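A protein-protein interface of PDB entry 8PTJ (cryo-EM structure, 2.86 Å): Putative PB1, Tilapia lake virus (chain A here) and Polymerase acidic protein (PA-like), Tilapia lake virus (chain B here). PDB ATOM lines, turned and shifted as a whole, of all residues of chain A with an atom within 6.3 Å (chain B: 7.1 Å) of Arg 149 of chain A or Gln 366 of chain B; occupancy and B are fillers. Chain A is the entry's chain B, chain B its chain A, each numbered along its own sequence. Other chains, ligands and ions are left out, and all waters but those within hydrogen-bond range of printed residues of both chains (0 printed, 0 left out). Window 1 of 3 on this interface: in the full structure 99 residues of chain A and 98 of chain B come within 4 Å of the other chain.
The backbone NH of Gly 11 of chain A lies within hydrogen-bond range of the side-chain sulfur of Cys 9 of chain A (3.3 Å).
O of Asn 12 of chain A sits at hydrogen-bond distance from NE of Arg 149 of chain A, at 3.2 Å.
NE of Arg 149 of chain A is in hydrogen-bond range of O of Leu 14 of chain A (2.5 Å).
The backbone carbonyl oxygen (O) of Gly 16 of chain A lies close to the side-chain amide oxygen (OE1) of Gln 147 of chain A, at 3.0 Å.
The backbone carbonyl oxygen (O) of Pro 17 of chain A is in hydrogen-bond range of the backbone NH (N) of Gln 147 of chain A, at 2.6 Å.
Hydrophobic or aromatic side chains of chain A within 4 Å of the printed part of chain B: Trp 2, Leu 14, Pro 17 and Pro 152.
Printed residues of chain B that touch a printed residue of chain A: Arg 359, Val 360, Ser 361, Gln 362, Ala 363, Val 364, Ala 365, Gln 366 and Asn 369.
Among the printed residues, no Asp or Glu carboxylate lies within 4 Å of a Lys or Arg side-chain nitrogen of the other chain.
Among the printed residues, pairs that only touch across the chains: Trp 2 of chain A with Ser 361 of chain B (3.9 Å), Trp 2 of chain A with Val 364 of chain B (3.6 Å), Trp 2 of chain A with Ala 365 of chain B (3.5 Å), Cys 9 of chain A with Asn 369 of chain B (3.6 Å), Lys 10 of chain A with Ala 365 of chain B (3.8 Å), Lys 10 of chain A with Gln 366 of chain B (3.9 Å), Lys 10 of chain A with Asn 369 of chain B (3.8 Å), Gly 11 of chain A with Gln 362 of chain B (3.2 Å), Gly 16 of chain A with Arg 359 of chain B (3.9 Å), Gly 16 of chain A with Gln 362 of chain B (3.99 Å), Pro 17 of chain A with Gln 362 of chain B (3.9 Å), Arg 149 of chain A with Gln 362 of chain B (3.5 Å), Gly 150 of chain A with Gln 362 of chain B (3.6 Å), Gly 150 of chain A with Ala 363 of chain B (3.5 Å), Gly 150 of chain A with Gln 366 of chain B (3.5 Å) and Pro 152 of chain A with Val 360 of chain B (3.9 Å).
NH1 of Arg 359 of chain B sits at hydrogen-bond distance from O of Ser 15 of chain A, 3.0 Å away.
The side-chain amide nitrogen (NE2) of Gln 362 of chain B lies within hydrogen-bond range of the backbone carbonyl oxygen (O) of Leu 14 of chain A.
O of Ser 15 of chain A sits at hydrogen-bond distance from NE2 of Gln 362 of chain B (2.9 Å).
The side-chain amide nitrogen (NE2) of Gln 366 of chain B lies within hydrogen-bond range of the backbone carbonyl oxygen (O) of Arg 149 of chain A.
Of the printed residues of chain B, Lys 10 of chain A touches Ala 365, Gln 366 and Asn 369.
Printed residues of chain B within 4 Å of Pro 17 of chain A: Gln 362 (3.9 Å).
Of chain B, only Gln 362 and Gln 366 come within 4 Å of Arg 149 of chain A.
Of the printed residues of chain A, Arg 359 of chain B touches Ser 15 and Gly 16.
Printed residues of chain A within 4 Å of Val 360 of chain B: Pro 152.
Of the printed residues of chain A, Ala 363 of chain B touches Gly 150 (3.5 Å).
Gln 366 of chain B touches three residues of chain A.
Tyr 386 of chain B touches none of the printed residues of chain A.
The nearest residue of chain B that does not touch Arg 149 of chain A is Ala 363 of chain B (5.5 Å).
The nearest residue of chain A that does not touch Gln 366 of chain B is Asn 12 of chain A (4.4 Å).
The nearest printed residue of chain A that does not touch Arg 359 of chain B is Pro 17 of chain A (4.1 Å).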
ATOM      1  N   TRP A   2     -12.420  22.497   6.848  1.00  0.00           N
ATOM      2  CA  TRP A   2     -13.537  22.404   7.780  1.00  0.00           C
ATOM      3  C   TRP A   2     -13.168  22.932   9.159  1.00  0.00           C
ATOM      4  O   TRP A   2     -14.059  23.331   9.916  1.00  0.00           O
ATOM      5  CB  TRP A   2     -14.017  20.955   7.894  1.00  0.00           C
ATOM      6  CG  TRP A   2     -12.903  19.963   8.030  1.00  0.00           C
ATOM      7  CD1 TRP A   2     -12.361  19.203   7.038  1.00  0.00           C
ATOM      8  CD2 TRP A   2     -12.189  19.630   9.226  1.00  0.00           C
ATOM      9  NE1 TRP A   2     -11.356  18.417   7.541  1.00  0.00           N
ATOM     10  CE2 TRP A   2     -11.230  18.660   8.882  1.00  0.00           C
ATOM     11  CE3 TRP A   2     -12.270  20.057  10.554  1.00  0.00           C
ATOM     12  CZ2 TRP A   2     -10.359  18.110   9.815  1.00  0.00           C
ATOM     13  CZ3 TRP A   2     -11.404  19.510  11.479  1.00  0.00           C
ATOM     14  CH2 TRP A   2     -10.461  18.547  11.106  1.00  0.00           C
ATOM     15  N   CYS A   9     -19.541  23.157  11.065  1.00  0.00           N
ATOM     16  CA  CYS A   9     -19.373  22.342   9.870  1.00  0.00           C
ATOM     17  C   CYS A   9     -18.963  20.936  10.279  1.00  0.00           C
ATOM     18  O   CYS A   9     -18.025  20.765  11.062  1.00  0.00           O
ATOM     19  CB  CYS A   9     -18.325  22.944   8.929  1.00  0.00           C
ATOM     20  SG  CYS A   9     -17.936  21.917   7.497  1.00  0.00           S
ATOM     21  N   LYS A  10     -19.664  19.938   9.749  1.00  0.00           N
ATOM     22  CA  LYS A  10     -19.366  18.541  10.028  1.00  0.00           C
ATOM     23  C   LYS A  10     -18.428  17.915   9.004  1.00  0.00           C
ATOM     24  O   LYS A  10     -18.093  16.734   9.136  1.00  0.00           O
ATOM     25  CB  LYS A  10     -20.664  17.730  10.088  1.00  0.00           C
ATOM     26  CG  LYS A  10     -21.230  17.581  11.489  1.00  0.00           C
ATOM     27  CD  LYS A  10     -22.749  17.520  11.485  1.00  0.00           C
ATOM     28  CE  LYS A  10     -23.327  17.969  12.817  1.00  0.00           C
ATOM     29  NZ  LYS A  10     -23.872  19.354  12.752  1.00  0.00           N
ATOM     30  N   GLY A  11     -17.996  18.668   7.998  1.00  0.00           N
ATOM     31  CA  GLY A  11     -17.113  18.119   6.983  1.00  0.00           C
ATOM     32  C   GLY A  11     -17.752  17.048   6.127  1.00  0.00           C
ATOM     33  O   GLY A  11     -17.126  16.012   5.869  1.00  0.00           O
ATOM     34  N   ASN A  12     -18.983  17.272   5.675  1.00  0.00           N
ATOM     35  CA  ASN A  12     -19.714  16.308   4.864  1.00  0.00           C
ATOM     36  C   ASN A  12     -19.565  16.559   3.369  1.00  0.00           C
ATOM     37  O   ASN A  12     -20.260  15.917   2.577  1.00  0.00           O
ATOM     38  CB  ASN A  12     -21.198  16.329   5.236  1.00  0.00           C
ATOM     39  CG  ASN A  12     -21.470  15.702   6.584  1.00  0.00           C
ATOM     40  OD1 ASN A  12     -20.574  15.147   7.217  1.00  0.00           O
ATOM     41  ND2 ASN A  12     -22.716  15.788   7.033  1.00  0.00           N
ATOM     42  N   LEU A  13     -18.685  17.475   2.965  1.00  0.00           N
ATOM     43  CA  LEU A  13     -18.592  17.841   1.559  1.00  0.00           C
ATOM     44  C   LEU A  13     -18.093  16.698   0.685  1.00  0.00           C
ATOM     45  O   LEU A  13     -18.367  16.694  -0.519  1.00  0.00           O
ATOM     46  CB  LEU A  13     -17.676  19.056   1.393  1.00  0.00           C
ATOM     47  CG  LEU A  13     -18.155  20.380   1.998  1.00  0.00           C
ATOM     48  CD1 LEU A  13     -17.459  21.575   1.361  1.00  0.00           C
ATOM     49  CD2 LEU A  13     -19.661  20.518   1.867  1.00  0.00           C
ATOM     50  N   LEU A  14     -17.374  15.736   1.252  1.00  0.00           N
ATOM     51  CA  LEU A  14     -16.904  14.573   0.514  1.00  0.00           C
ATOM     52  C   LEU A  14     -17.761  13.356   0.844  1.00  0.00           C
ATOM     53  O   LEU A  14     -18.457  13.312   1.859  1.00  0.00           O
ATOM     54  CB  LEU A  14     -15.435  14.282   0.833  1.00  0.00           C
ATOM     55  CG  LEU A  14     -14.433  15.381   0.476  1.00  0.00           C
ATOM     56  CD1 LEU A  14     -13.035  14.984   0.911  1.00  0.00           C
ATOM     57  CD2 LEU A  14     -14.461  15.683  -1.011  1.00  0.00           C
ATOM     58  N   SER A  15     -17.699  12.361  -0.035  1.00  0.00           N
ATOM     59  CA  SER A  15     -18.478  11.148   0.151  1.00  0.00           C
ATOM     60  C   SER A  15     -17.976  10.374   1.368  1.00  0.00           C
ATOM     61  O   SER A  15     -16.896  10.633   1.906  1.00  0.00           O
ATOM     62  CB  SER A  15     -18.409  10.270  -1.096  1.00  0.00           C
ATOM     63  OG  SER A  15     -18.737  11.007  -2.259  1.00  0.00           O
ATOM     64  N   GLY A  16     -18.780   9.410   1.801  1.00  0.00           N
ATOM     65  CA  GLY A  16     -18.430   8.581   2.928  1.00  0.00           C
ATOM     66  C   GLY A  16     -17.362   7.569   2.574  1.00  0.00           C
ATOM     67  O   GLY A  16     -17.031   7.363   1.402  1.00  0.00           O
ATOM     68  N   PRO A  17     -16.796   6.917   3.585  1.00  0.00           N
ATOM     69  CA  PRO A  17     -15.738   5.937   3.326  1.00  0.00           C
ATOM     70  C   PRO A  17     -16.266   4.697   2.627  1.00  0.00           C
ATOM     71  O   PRO A  17     -17.441   4.339   2.740  1.00  0.00           O
ATOM     72  CB  PRO A  17     -15.215   5.602   4.727  1.00  0.00           C
ATOM     73  CG  PRO A  17     -16.343   5.908   5.637  1.00  0.00           C
ATOM     74  CD  PRO A  17     -17.100   7.042   5.020  1.00  0.00           C
ATOM     75  N   GLN A 147     -19.778   3.777   3.598  1.00  0.00           N
ATOM     76  CA  GLN A 147     -20.282   5.056   3.099  1.00  0.00           C
ATOM     77  C   GLN A 147     -21.029   5.813   4.195  1.00  0.00           C
ATOM     78  O   GLN A 147     -22.038   6.474   3.943  1.00  0.00           O
ATOM     79  CB  GLN A 147     -21.172   4.858   1.869  1.00  0.00           C
ATOM     80  CG  GLN A 147     -20.399   4.574   0.592  1.00  0.00           C
ATOM     81  CD  GLN A 147     -20.195   5.813  -0.258  1.00  0.00           C
ATOM     82  OE1 GLN A 147     -19.064   6.204  -0.546  1.00  0.00           O
ATOM     83  NE2 GLN A 147     -21.294   6.435  -0.672  1.00  0.00           N
ATOM     84  N   GLU A 148     -20.523   5.717   5.422  1.00  0.00           N
ATOM     85  CA  GLU A 148     -21.049   6.461   6.563  1.00  0.00           C
ATOM     86  C   GLU A 148     -19.992   7.465   6.999  1.00  0.00           C
ATOM     87  O   GLU A 148     -18.938   7.080   7.513  1.00  0.00           O
ATOM     88  CB  GLU A 148     -21.415   5.524   7.710  1.00  0.00           C
ATOM     89  CG  GLU A 148     -22.881   5.157   7.751  1.00  0.00           C
ATOM     90  CD  GLU A 148     -23.211   4.222   8.891  1.00  0.00           C
ATOM     91  OE1 GLU A 148     -24.157   3.425   8.743  1.00  0.00           O
ATOM     92  OE2 GLU A 148     -22.523   4.279   9.931  1.00  0.00           O
ATOM     93  N   ARG A 149     -20.277   8.747   6.797  1.00  0.00           N
ATOM     94  CA  ARG A 149     -19.314   9.784   7.134  1.00  0.00           C
ATOM     95  C   ARG A 149     -18.966   9.726   8.615  1.00  0.00           C
ATOM     96  O   ARG A 149     -19.841   9.568   9.471  1.00  0.00           O
ATOM     97  CB  ARG A 149     -19.877  11.158   6.775  1.00  0.00           C
ATOM     98  CG  ARG A 149     -20.318  11.278   5.329  1.00  0.00           C
ATOM     99  CD  ARG A 149     -20.136  12.690   4.806  1.00  0.00           C
ATOM    100  NE  ARG A 149     -20.401  12.783   3.376  1.00  0.00           N
ATOM    101  CZ  ARG A 149     -21.606  12.702   2.829  1.00  0.00           C
ATOM    102  NH1 ARG A 149     -22.690  12.525   3.566  1.00  0.00           N
ATOM    103  NH2 ARG A 149     -21.727  12.804   1.509  1.00  0.00           N
ATOM    104  N   GLY A 150     -17.676   9.854   8.913  1.00  0.00           N
ATOM    105  CA  GLY A 150     -17.208   9.823  10.282  1.00  0.00           C
ATOM    106  C   GLY A 150     -16.965   8.444  10.847  1.00  0.00           C
ATOM    107  O   GLY A 150     -16.730   8.322  12.054  1.00  0.00           O
ATOM    108  N   LYS A 151     -17.012   7.401  10.021  1.00  0.00           N
ATOM    109  CA  LYS A 151     -16.812   6.021  10.462  1.00  0.00           C
ATOM    110  C   LYS A 151     -15.749   5.382   9.580  1.00  0.00           C
ATOM    111  O   LYS A 151     -16.066   4.629   8.650  1.00  0.00           O
ATOM    112  CB  LYS A 151     -18.119   5.229  10.412  1.00  0.00           C
ATOM    113  CG  LYS A 151     -19.229   5.812  11.269  1.00  0.00           C
ATOM    114  CD  LYS A 151     -19.381   5.051  12.574  1.00  0.00           C
ATOM    115  CE  LYS A 151     -20.627   5.486  13.331  1.00  0.00           C
ATOM    116  NZ  LYS A 151     -20.362   6.649  14.223  1.00  0.00           N
ATOM    117  N   PRO A 152     -14.470   5.665   9.842  1.00  0.00           N
ATOM    118  CA  PRO A 152     -13.414   5.068   9.007  1.00  0.00           C
ATOM    119  C   PRO A 152     -13.463   3.552   8.981  1.00  0.00           C
ATOM    120  O   PRO A 152     -13.199   2.943   7.938  1.00  0.00           O
ATOM    121  CB  PRO A 152     -12.121   5.587   9.653  1.00  0.00           C
ATOM    122  CG  PRO A 152     -12.529   6.770  10.458  1.00  0.00           C
ATOM    123  CD  PRO A 152     -13.922   6.511  10.913  1.00  0.00           C
ATOM    124  N   CYS A 346     -24.728  20.480   8.039  1.00  0.00           N
ATOM    125  CA  CYS A 346     -24.779  19.138   7.478  1.00  0.00           C
ATOM    126  C   CYS A 346     -24.728  19.131   5.956  1.00  0.00           C
ATOM    127  O   CYS A 346     -24.967  18.084   5.347  1.00  0.00           O
ATOM    128  CB  CYS A 346     -26.042  18.421   7.956  1.00  0.00           C
ATOM    129  SG  CYS A 346     -25.944  17.817   9.649  1.00  0.00           S
ATOM    130  N   ALA A 348     -23.810  18.549   2.325  1.00  0.00           N
ATOM    131  CA  ALA A 348     -23.008  17.493   1.728  1.00  0.00           C
ATOM    132  C   ALA A 348     -22.796  17.780   0.250  1.00  0.00           C
ATOM    133  O   ALA A 348     -23.682  18.315  -0.422  1.00  0.00           O
ATOM    134  CB  ALA A 348     -23.674  16.125   1.901  1.00  0.00           C
ATOM    135  N   GLY A 349     -21.616  17.422  -0.251  1.00  0.00           N
ATOM    136  CA  GLY A 349     -21.311  17.614  -1.650  1.00  0.00           C
ATOM    137  C   GLY A 349     -21.998  16.595  -2.536  1.00  0.00           C
ATOM    138  O   GLY A 349     -22.509  15.572  -2.084  1.00  0.00           O
ATOM    139  N   PRO A 351     -21.270  14.115  -5.567  1.00  0.00           N
ATOM    140  CA  PRO A 351     -20.257  13.486  -6.418  1.00  0.00           C
ATOM    141  C   PRO A 351     -20.727  13.383  -7.860  1.00  0.00           C
ATOM    142  O   PRO A 351     -21.921  13.421  -8.164  1.00  0.00           O
ATOM    143  CB  PRO A 351     -20.072  12.101  -5.792  1.00  0.00           C
ATOM    144  CG  PRO A 351     -21.355  11.822  -5.110  1.00  0.00           C
ATOM    145  CD  PRO A 351     -21.903  13.143  -4.658  1.00  0.00           C
ATOM    146  N   ARG B 359     -11.574   8.409   4.687  1.00  0.00           N
ATOM    147  CA  ARG B 359     -12.191   9.666   5.103  1.00  0.00           C
ATOM    148  C   ARG B 359     -12.149   9.829   6.621  1.00  0.00           C
ATOM    149  O   ARG B 359     -13.143  10.169   7.264  1.00  0.00           O
ATOM    150  CB  ARG B 359     -13.625   9.762   4.583  1.00  0.00           C
ATOM    151  CG  ARG B 359     -13.756   9.603   3.076  1.00  0.00           C
ATOM    152  CD  ARG B 359     -13.512  10.914   2.355  1.00  0.00           C
ATOM    153  NE  ARG B 359     -12.827  10.724   1.082  1.00  0.00           N
ATOM    154  CZ  ARG B 359     -13.421  10.344  -0.041  1.00  0.00           C
ATOM    155  NH1 ARG B 359     -14.719  10.103  -0.091  1.00  0.00           N
ATOM    156  NH2 ARG B 359     -12.691  10.207  -1.145  1.00  0.00           N
ATOM    157  N   VAL B 360     -10.973   9.576   7.201  1.00  0.00           N
ATOM    158  CA  VAL B 360     -10.800   9.778   8.638  1.00  0.00           C
ATOM    159  C   VAL B 360     -10.949  11.251   8.990  1.00  0.00           C
ATOM    160  O   VAL B 360     -11.366  11.599  10.107  1.00  0.00           O
ATOM    161  CB  VAL B 360      -9.434   9.220   9.088  1.00  0.00           C
ATOM    162  CG1 VAL B 360      -8.299  10.005   8.454  1.00  0.00           C
ATOM    163  CG2 VAL B 360      -9.324   9.239  10.603  1.00  0.00           C
ATOM    164  N   SER B 361     -10.615  12.139   8.052  1.00  0.00           N
ATOM    165  CA  SER B 361     -10.804  13.563   8.287  1.00  0.00           C
ATOM    166  C   SER B 361     -12.252  13.882   8.621  1.00  0.00           C
ATOM    167  O   SER B 361     -12.519  14.840   9.347  1.00  0.00           O
ATOM    168  CB  SER B 361     -10.352  14.360   7.064  1.00  0.00           C
ATOM    169  OG  SER B 361     -11.271  14.224   5.996  1.00  0.00           O
ATOM    170  N   GLN B 362     -13.201  13.093   8.112  1.00  0.00           N
ATOM    171  CA  GLN B 362     -14.600  13.311   8.464  1.00  0.00           C
ATOM    172  C   GLN B 362     -14.845  13.057   9.946  1.00  0.00           C
ATOM    173  O   GLN B 362     -15.545  13.833  10.607  1.00  0.00           O
ATOM    174  CB  GLN B 362     -15.500  12.415   7.614  1.00  0.00           C
ATOM    175  CG  GLN B 362     -16.041  13.090   6.370  1.00  0.00           C
ATOM    176  CD  GLN B 362     -16.377  12.104   5.274  1.00  0.00           C
ATOM    177  OE1 GLN B 362     -16.479  10.903   5.515  1.00  0.00           O
ATOM    178  NE2 GLN B 362     -16.553  12.607   4.061  1.00  0.00           N
ATOM    179  N   ALA B 363     -14.277  11.977  10.487  1.00  0.00           N
ATOM    180  CA  ALA B 363     -14.415  11.714  11.916  1.00  0.00           C
ATOM    181  C   ALA B 363     -13.736  12.800  12.738  1.00  0.00           C
ATOM    182  O   ALA B 363     -14.274  13.251  13.759  1.00  0.00           O
ATOM    183  CB  ALA B 363     -13.834  10.343  12.255  1.00  0.00           C
ATOM    184  N   VAL B 364     -12.551  13.238  12.306  1.00  0.00           N
ATOM    185  CA  VAL B 364     -11.868  14.310  13.022  1.00  0.00           C
ATOM    186  C   VAL B 364     -12.713  15.578  13.006  1.00  0.00           C
ATOM    187  O   VAL B 364     -12.820  16.283  14.014  1.00  0.00           O
ATOM    188  CB  VAL B 364     -10.469  14.554  12.425  1.00  0.00           C
ATOM    189  CG1 VAL B 364      -9.760  15.668  13.177  1.00  0.00           C
ATOM    190  CG2 VAL B 364      -9.644  13.283  12.469  1.00  0.00           C
ATOM    191  N   ALA B 365     -13.323  15.888  11.860  1.00  0.00           N
ATOM    192  CA  ALA B 365     -14.154  17.081  11.751  1.00  0.00           C
ATOM    193  C   ALA B 365     -15.385  16.983  12.637  1.00  0.00           C
ATOM    194  O   ALA B 365     -15.784  17.971  13.261  1.00  0.00           O
ATOM    195  CB  ALA B 365     -14.564  17.299  10.296  1.00  0.00           C
ATOM    196  N   GLN B 366     -16.013  15.808  12.695  1.00  0.00           N
ATOM    197  CA  GLN B 366     -17.173  15.644  13.565  1.00  0.00           C
ATOM    198  C   GLN B 366     -16.791  15.838  15.026  1.00  0.00           C
ATOM    199  O   GLN B 366     -17.499  16.524  15.780  1.00  0.00           O
ATOM    200  CB  GLN B 366     -17.796  14.267  13.348  1.00  0.00           C
ATOM    201  CG  GLN B 366     -18.539  14.137  12.033  1.00  0.00           C
ATOM    202  CD  GLN B 366     -19.037  12.733  11.780  1.00  0.00           C
ATOM    203  OE1 GLN B 366     -19.035  11.891  12.676  1.00  0.00           O
ATOM    204  NE2 GLN B 366     -19.469  12.471  10.554  1.00  0.00           N
ATOM    205  N   HIS B 367     -15.666  15.258  15.446  1.00  0.00           N
ATOM    206  CA  HIS B 367     -15.248  15.433  16.832  1.00  0.00           C
ATOM    207  C   HIS B 367     -14.875  16.882  17.118  1.00  0.00           C
ATOM    208  O   HIS B 367     -15.147  17.391  18.208  1.00  0.00           O
ATOM    209  CB  HIS B 367     -14.082  14.507  17.165  1.00  0.00           C
ATOM    210  CG  HIS B 367     -13.958  14.210  18.627  1.00  0.00           C
ATOM    211  ND1 HIS B 367     -14.962  13.599  19.347  1.00  0.00           N
ATOM    212  CD2 HIS B 367     -12.958  14.451  19.505  1.00  0.00           C
ATOM    213  CE1 HIS B 367     -14.582  13.471  20.604  1.00  0.00           C
ATOM    214  NE2 HIS B 367     -13.370  13.979  20.728  1.00  0.00           N
ATOM    215  N   PHE B 368     -14.254  17.565  16.157  1.00  0.00           N
ATOM    216  CA  PHE B 368     -13.922  18.972  16.357  1.00  0.00           C
ATOM    217  C   PHE B 368     -15.178  19.828  16.439  1.00  0.00           C
ATOM    218  O   PHE B 368     -15.227  20.800  17.200  1.00  0.00           O
ATOM    219  CB  PHE B 368     -13.010  19.460  15.233  1.00  0.00           C
ATOM    220  CG  PHE B 368     -12.473  20.844  15.446  1.00  0.00           C
ATOM    221  CD1 PHE B 368     -11.769  21.160  16.595  1.00  0.00           C
ATOM    222  CD2 PHE B 368     -12.670  21.830  14.497  1.00  0.00           C
ATOM    223  CE1 PHE B 368     -11.277  22.433  16.793  1.00  0.00           C
ATOM    224  CE2 PHE B 368     -12.179  23.104  14.691  1.00  0.00           C
ATOM    225  CZ  PHE B 368     -11.480  23.405  15.839  1.00  0.00           C
ATOM    226  N   ASN B 369     -16.200  19.491  15.651  1.00  0.00           N
ATOM    227  CA  ASN B 369     -17.474  20.191  15.752  1.00  0.00           C
ATOM    228  C   ASN B 369     -18.090  19.997  17.129  1.00  0.00           C
ATOM    229  O   ASN B 369     -18.624  20.942  17.720  1.00  0.00           O
ATOM    230  CB  ASN B 369     -18.429  19.699  14.666  1.00  0.00           C
ATOM    231  CG  ASN B 369     -19.727  20.475  14.636  1.00  0.00           C
ATOM    232  OD1 ASN B 369     -19.743  21.668  14.338  1.00  0.00           O
ATOM    233  ND2 ASN B 369     -20.825  19.802  14.951  1.00  0.00           N
ATOM    234  N   ARG B 370     -18.027  18.774  17.658  1.00  0.00           N
ATOM    235  CA  ARG B 370     -18.478  18.551  19.029  1.00  0.00           C
ATOM    236  C   ARG B 370     -17.658  19.380  20.009  1.00  0.00           C
ATOM    237  O   ARG B 370     -18.197  19.944  20.968  1.00  0.00           O
ATOM    238  CB  ARG B 370     -18.386  17.068  19.379  1.00  0.00           C
ATOM    239  CG  ARG B 370     -19.502  16.224  18.799  1.00  0.00           C
ATOM    240  CD  ARG B 370     -19.534  14.848  19.435  1.00  0.00           C
ATOM    241  NE  ARG B 370     -18.470  13.987  18.933  1.00  0.00           N
ATOM    242  CZ  ARG B 370     -18.558  13.239  17.842  1.00  0.00           C
ATOM    243  NH1 ARG B 370     -19.656  13.219  17.103  1.00  0.00           N
ATOM    244  NH2 ARG B 370     -17.520  12.492  17.484  1.00  0.00           N
ATOM    245  N   HIS B 371     -16.346  19.459  19.782  1.00  0.00           N
ATOM    246  CA  HIS B 371     -15.461  20.202  20.671  1.00  0.00           C
ATOM    247  C   HIS B 371     -15.816  21.683  20.701  1.00  0.00           C
ATOM    248  O   HIS B 371     -15.848  22.301  21.772  1.00  0.00           O
ATOM    249  CB  HIS B 371     -14.014  19.999  20.217  1.00  0.00           C
ATOM    250  CG  HIS B 371     -12.994  20.663  21.088  1.00  0.00           C
ATOM    251  ND1 HIS B 371     -11.647  20.636  20.798  1.00  0.00           N
ATOM    252  CD2 HIS B 371     -13.117  21.365  22.238  1.00  0.00           C
ATOM    253  CE1 HIS B 371     -10.986  21.296  21.732  1.00  0.00           C
ATOM    254  NE2 HIS B 371     -11.854  21.748  22.617  1.00  0.00           N
ATOM    255  N   ARG B 372     -16.089  22.272  19.537  1.00  0.00           N
ATOM    256  CA  ARG B 372     -16.322  23.710  19.466  1.00  0.00           C
ATOM    257  C   ARG B 372     -17.638  24.122  20.107  1.00  0.00           C
ATOM    258  O   ARG B 372     -17.776  25.281  20.511  1.00  0.00           O
ATOM    259  CB  ARG B 372     -16.292  24.172  18.011  1.00  0.00           C
ATOM    260  CG  ARG B 372     -14.892  24.380  17.461  1.00  0.00           C
ATOM    261  CD  ARG B 372     -14.871  25.446  16.382  1.00  0.00           C
ATOM    262  NE  ARG B 372     -15.505  24.985  15.153  1.00  0.00           N
ATOM    263  CZ  ARG B 372     -16.100  25.774  14.270  1.00  0.00           C
ATOM    264  NH1 ARG B 372     -16.167  27.084  14.443  1.00  0.00           N
ATOM    265  NH2 ARG B 372     -16.643  25.235  13.183  1.00  0.00           N
ATOM    266  N   PHE B 382     -13.405  12.243  26.200  1.00  0.00           N
ATOM    267  CA  PHE B 382     -13.555  13.087  25.021  1.00  0.00           C
ATOM    268  C   PHE B 382     -12.210  13.315  24.346  1.00  0.00           C
ATOM    269  O   PHE B 382     -12.119  13.329  23.113  1.00  0.00           O
ATOM    270  CB  PHE B 382     -14.196  14.417  25.409  1.00  0.00           C
ATOM    271  CG  PHE B 382     -14.518  15.298  24.240  1.00  0.00           C
ATOM    272  CD1 PHE B 382     -13.567  16.158  23.721  1.00  0.00           C
ATOM    273  CD2 PHE B 382     -15.773  15.270  23.662  1.00  0.00           C
ATOM    274  CE1 PHE B 382     -13.860  16.968  22.648  1.00  0.00           C
ATOM    275  CE2 PHE B 382     -16.073  16.079  22.588  1.00  0.00           C
ATOM    276  CZ  PHE B 382     -15.115  16.929  22.080  1.00  0.00           C
ATOM    277  N   TYR B 386      -9.755  11.998  19.318  1.00  0.00           N
ATOM    278  CA  TYR B 386      -8.794  12.322  18.278  1.00  0.00           C
ATOM    279  C   TYR B 386      -7.765  11.220  18.069  1.00  0.00           C
ATOM    280  O   TYR B 386      -6.941  11.327  17.156  1.00  0.00           O
ATOM    281  CB  TYR B 386      -8.077  13.630  18.622  1.00  0.00           C
ATOM    282  CG  TYR B 386      -8.995  14.827  18.710  1.00  0.00           C
ATOM    283  CD1 TYR B 386      -9.617  15.334  17.579  1.00  0.00           C
ATOM    284  CD2 TYR B 386      -9.237  15.450  19.925  1.00  0.00           C
ATOM    285  CE1 TYR B 386     -10.453  16.427  17.655  1.00  0.00           C
ATOM    286  CE2 TYR B 386     -10.073  16.544  20.010  1.00  0.00           C
ATOM    287  CZ  TYR B 386     -10.678  17.027  18.872  1.00  0.00           C
ATOM    288  OH  TYR B 386     -11.510  18.117  18.953  1.00  0.00           O
